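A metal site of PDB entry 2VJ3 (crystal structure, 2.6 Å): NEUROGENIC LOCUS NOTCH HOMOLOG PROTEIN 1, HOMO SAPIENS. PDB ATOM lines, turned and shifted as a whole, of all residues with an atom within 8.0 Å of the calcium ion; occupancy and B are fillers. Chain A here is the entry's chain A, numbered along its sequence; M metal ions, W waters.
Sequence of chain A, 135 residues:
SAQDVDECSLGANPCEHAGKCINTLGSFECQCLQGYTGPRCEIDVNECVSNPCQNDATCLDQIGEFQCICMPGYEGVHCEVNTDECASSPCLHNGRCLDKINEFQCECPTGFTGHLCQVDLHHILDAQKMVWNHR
Water W1 lies within hydrogen-bond range of the side-chain carboxylate (OE2) of Glu 7 and the backbone carbonyl oxygen (O) of Gly 26.
The backbone carbonyl oxygen (O) of Ser 27 sits close to the side-chain hydroxyl (OG1) of Thr 24 (3.1 Å).
SG of Cys 8 sits at hydrogen-bond distance from N of Asn 23 (3.6 Å).
The backbone NH of Phe 28 is in hydrogen-bond range of the side-chain hydroxyl of Thr 24 (3.3 Å).
The side-chain carboxylate (OD1) of Asp 4 lies close to the backbone NH (N) of Gly 26 (2.9 Å).
The calcium ion is bound by the backbone carbonyl oxygen of Ser 27 (2.4 Å), the side-chain amide oxygen of Asn 23 (2.4 Å), water W1 (2.5 Å), the side-chain carboxylate of Glu 7 (2.6 Å), the backbone carbonyl oxygen of Thr 24 (2.6 Å), the backbone carbonyl oxygen of Val 5 (2.6 Å) and the side-chain carboxylate of Asp 4 (2.8 Å).
Six residues have an atom within 4 Å of the calcium ion: Asp 4, Val 5, Glu 7, Asn 23, Thr 24 and Ser 27.
The nearest printed residue that does not touch the calcium ion is Gly 26 (4.2 Å).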
ATOM      1  N   GLN A   3       2.428  31.281 -13.831  1.00  0.00           N
ATOM      2  CA  GLN A   3       1.004  31.008 -14.177  1.00  0.00           C
ATOM      3  C   GLN A   3       0.906  29.937 -15.260  1.00  0.00           C
ATOM      4  O   GLN A   3       1.654  29.954 -16.237  1.00  0.00           O
ATOM      5  CB  GLN A   3       0.294  32.285 -14.612  1.00  0.00           C
ATOM      6  CG  GLN A   3      -1.219  32.153 -14.815  1.00  0.00           C
ATOM      7  CD  GLN A   3      -1.959  31.721 -13.558  1.00  0.00           C
ATOM      8  OE1 GLN A   3      -1.611  32.117 -12.440  1.00  0.00           O
ATOM      9  NE2 GLN A   3      -3.006  30.917 -13.733  1.00  0.00           N
ATOM     10  N   ASP A   4      -0.035  29.015 -15.073  1.00  0.00           N
ATOM     11  CA  ASP A   4      -0.246  27.915 -16.007  1.00  0.00           C
ATOM     12  C   ASP A   4      -1.676  27.894 -16.544  1.00  0.00           C
ATOM     13  O   ASP A   4      -2.630  28.107 -15.794  1.00  0.00           O
ATOM     14  CB  ASP A   4       0.089  26.577 -15.336  1.00  0.00           C
ATOM     15  CG  ASP A   4      -0.068  25.384 -16.269  1.00  0.00           C
ATOM     16  OD1 ASP A   4       0.494  25.423 -17.386  1.00  0.00           O
ATOM     17  OD2 ASP A   4      -0.745  24.416 -15.879  1.00  0.00           O
ATOM     18  N   VAL A   5      -1.807  27.632 -17.838  1.00  0.00           N
ATOM     19  CA  VAL A   5      -3.103  27.477 -18.491  1.00  0.00           C
ATOM     20  C   VAL A   5      -3.393  25.997 -18.778  1.00  0.00           C
ATOM     21  O   VAL A   5      -2.551  25.296 -19.348  1.00  0.00           O
ATOM     22  CB  VAL A   5      -3.233  28.368 -19.767  1.00  0.00           C
ATOM     23  CG1 VAL A   5      -2.114  28.067 -20.778  1.00  0.00           C
ATOM     24  CG2 VAL A   5      -4.610  28.222 -20.421  1.00  0.00           C
ATOM     25  N   ASP A   6      -4.558  25.534 -18.360  1.00  0.00           N
ATOM     26  CA  ASP A   6      -4.977  24.156 -18.575  1.00  0.00           C
ATOM     27  C   ASP A   6      -5.516  23.981 -19.996  1.00  0.00           C
ATOM     28  O   ASP A   6      -6.675  24.294 -20.276  1.00  0.00           O
ATOM     29  CB  ASP A   6      -6.041  23.743 -17.540  1.00  0.00           C
ATOM     30  CG  ASP A   6      -6.387  22.262 -17.587  1.00  0.00           C
ATOM     31  OD1 ASP A   6      -5.875  21.533 -18.473  1.00  0.00           O
ATOM     32  OD2 ASP A   6      -7.176  21.818 -16.726  1.00  0.00           O
ATOM     33  N   GLU A   7      -4.660  23.473 -20.887  1.00  0.00           N
ATOM     34  CA  GLU A   7      -5.012  23.258 -22.289  1.00  0.00           C
ATOM     35  C   GLU A   7      -6.105  22.202 -22.481  1.00  0.00           C
ATOM     36  O   GLU A   7      -6.821  22.228 -23.486  1.00  0.00           O
ATOM     37  CB  GLU A   7      -3.782  22.876 -23.108  1.00  0.00           C
ATOM     38  CG  GLU A   7      -2.854  24.034 -23.460  1.00  0.00           C
ATOM     39  CD  GLU A   7      -1.802  24.304 -22.391  1.00  0.00           C
ATOM     40  OE1 GLU A   7      -1.674  23.505 -21.444  1.00  0.00           O
ATOM     41  OE2 GLU A   7      -1.079  25.313 -22.524  1.00  0.00           O
ATOM     42  N   CYS A   8      -6.223  21.297 -21.516  1.00  0.00           N
ATOM     43  CA  CYS A   8      -7.213  20.231 -21.556  1.00  0.00           C
ATOM     44  C   CYS A   8      -8.622  20.739 -21.246  1.00  0.00           C
ATOM     45  O   CYS A   8      -9.599  20.238 -21.779  1.00  0.00           O
ATOM     46  CB  CYS A   8      -6.827  19.110 -20.587  1.00  0.00           C
ATOM     47  SG  CYS A   8      -5.138  18.495 -20.802  1.00  0.00           S
ATOM     48  N   ILE A  22      -3.793  15.172 -20.425  1.00  0.00           N
ATOM     49  CA  ILE A  22      -3.237  15.365 -19.086  1.00  0.00           C
ATOM     50  C   ILE A  22      -2.483  16.691 -19.043  1.00  0.00           C
ATOM     51  O   ILE A  22      -1.520  16.891 -19.790  1.00  0.00           O
ATOM     52  CB  ILE A  22      -2.331  14.185 -18.675  1.00  0.00           C
ATOM     53  CG1 ILE A  22      -3.138  12.884 -18.593  1.00  0.00           C
ATOM     54  CG2 ILE A  22      -1.657  14.474 -17.330  1.00  0.00           C
ATOM     55  CD1 ILE A  22      -2.298  11.621 -18.616  1.00  0.00           C
ATOM     56  N   ASN A  23      -2.930  17.584 -18.169  1.00  0.00           N
ATOM     57  CA  ASN A  23      -2.337  18.903 -18.035  1.00  0.00           C
ATOM     58  C   ASN A  23      -1.016  18.877 -17.263  1.00  0.00           C
ATOM     59  O   ASN A  23      -0.903  18.205 -16.238  1.00  0.00           O
ATOM     60  CB  ASN A  23      -3.325  19.847 -17.354  1.00  0.00           C
ATOM     61  CG  ASN A  23      -2.807  21.275 -17.265  1.00  0.00           C
ATOM     62  OD1 ASN A  23      -2.184  21.780 -18.199  1.00  0.00           O
ATOM     63  ND2 ASN A  23      -3.074  21.923 -16.143  1.00  0.00           N
ATOM     64  N   THR A  24      -0.026  19.600 -17.786  1.00  0.00           N
ATOM     65  CA  THR A  24       1.244  19.805 -17.083  1.00  0.00           C
ATOM     66  C   THR A  24       1.488  21.296 -16.872  1.00  0.00           C
ATOM     67  O   THR A  24       0.779  22.140 -17.430  1.00  0.00           O
ATOM     68  CB  THR A  24       2.451  19.172 -17.826  1.00  0.00           C
ATOM     69  OG1 THR A  24       2.646  19.827 -19.081  1.00  0.00           O
ATOM     70  CG2 THR A  24       2.222  17.688 -18.065  1.00  0.00           C
ATOM     71  N   LEU A  25       2.480  21.629 -16.056  1.00  0.00           N
ATOM     72  CA  LEU A  25       2.855  23.024 -15.815  1.00  0.00           C
ATOM     73  C   LEU A  25       3.731  23.548 -16.944  1.00  0.00           C
ATOM     74  O   LEU A  25       4.882  23.147 -17.088  1.00  0.00           O
ATOM     75  CB  LEU A  25       3.569  23.180 -14.462  1.00  0.00           C
ATOM     76  CG  LEU A  25       2.791  22.898 -13.165  1.00  0.00           C
ATOM     77  CD1 LEU A  25       3.750  22.890 -11.982  1.00  0.00           C
ATOM     78  CD2 LEU A  25       1.660  23.902 -12.942  1.00  0.00           C
ATOM     79  N   GLY A  26       3.155  24.432 -17.760  1.00  0.00           N
ATOM     80  CA  GLY A  26       3.865  25.015 -18.902  1.00  0.00           C
ATOM     81  C   GLY A  26       3.395  24.479 -20.237  1.00  0.00           C
ATOM     82  O   GLY A  26       3.455  25.186 -21.247  1.00  0.00           O
ATOM     83  N   SER A  27       2.916  23.239 -20.244  1.00  0.00           N
ATOM     84  CA  SER A  27       2.447  22.595 -21.465  1.00  0.00           C
ATOM     85  C   SER A  27       1.318  21.599 -21.177  1.00  0.00           C
ATOM     86  O   SER A  27       0.526  21.807 -20.258  1.00  0.00           O
ATOM     87  CB  SER A  27       3.621  21.910 -22.165  1.00  0.00           C
ATOM     88  OG  SER A  27       3.265  21.477 -23.467  1.00  0.00           O
ATOM     89  N   PHE A  28       1.254  20.537 -21.954  1.00  0.00           N
ATOM     90  CA  PHE A  28       0.297  19.446 -21.747  1.00  0.00           C
ATOM     91  C   PHE A  28       0.809  18.166 -22.419  1.00  0.00           C
ATOM     92  O   PHE A  28       1.732  18.205 -23.232  1.00  0.00           O
ATOM     93  CB  PHE A  28      -1.096  19.814 -22.278  1.00  0.00           C
ATOM     94  CG  PHE A  28      -1.182  19.882 -23.786  1.00  0.00           C
ATOM     95  CD1 PHE A  28      -1.595  18.774 -24.518  1.00  0.00           C
ATOM     96  CD2 PHE A  28      -0.873  21.056 -24.470  1.00  0.00           C
ATOM     97  CE1 PHE A  28      -1.673  18.828 -25.911  1.00  0.00           C
ATOM     98  CE2 PHE A  28      -0.952  21.127 -25.853  1.00  0.00           C
ATOM     99  CZ  PHE A  28      -1.357  20.013 -26.574  1.00  0.00           C
ATOM    100  N   GLU A  29       0.217  17.038 -22.052  1.00  0.00           N
ATOM    101  CA  GLU A  29       0.563  15.754 -22.656  1.00  0.00           C
ATOM    102  C   GLU A  29      -0.680  14.925 -22.992  1.00  0.00           C
ATOM    103  O   GLU A  29      -1.727  15.080 -22.363  1.00  0.00           O
ATOM    104  CB  GLU A  29       1.516  14.953 -21.758  1.00  0.00           C
ATOM    105  CG  GLU A  29       1.015  14.715 -20.342  1.00  0.00           C
ATOM    106  CD  GLU A  29       2.082  14.148 -19.410  1.00  0.00           C
ATOM    107  OE1 GLU A  29       3.289  14.365 -19.663  1.00  0.00           O
ATOM    108  OE2 GLU A  29       1.703  13.479 -18.427  1.00  0.00           O
HETATM  109 CA    CA M   1      -0.695  23.500 -19.075  1.00  0.00          CA
HETATM  110  O   HOH W   1       0.417  25.667 -19.786  1.00  0.00           O
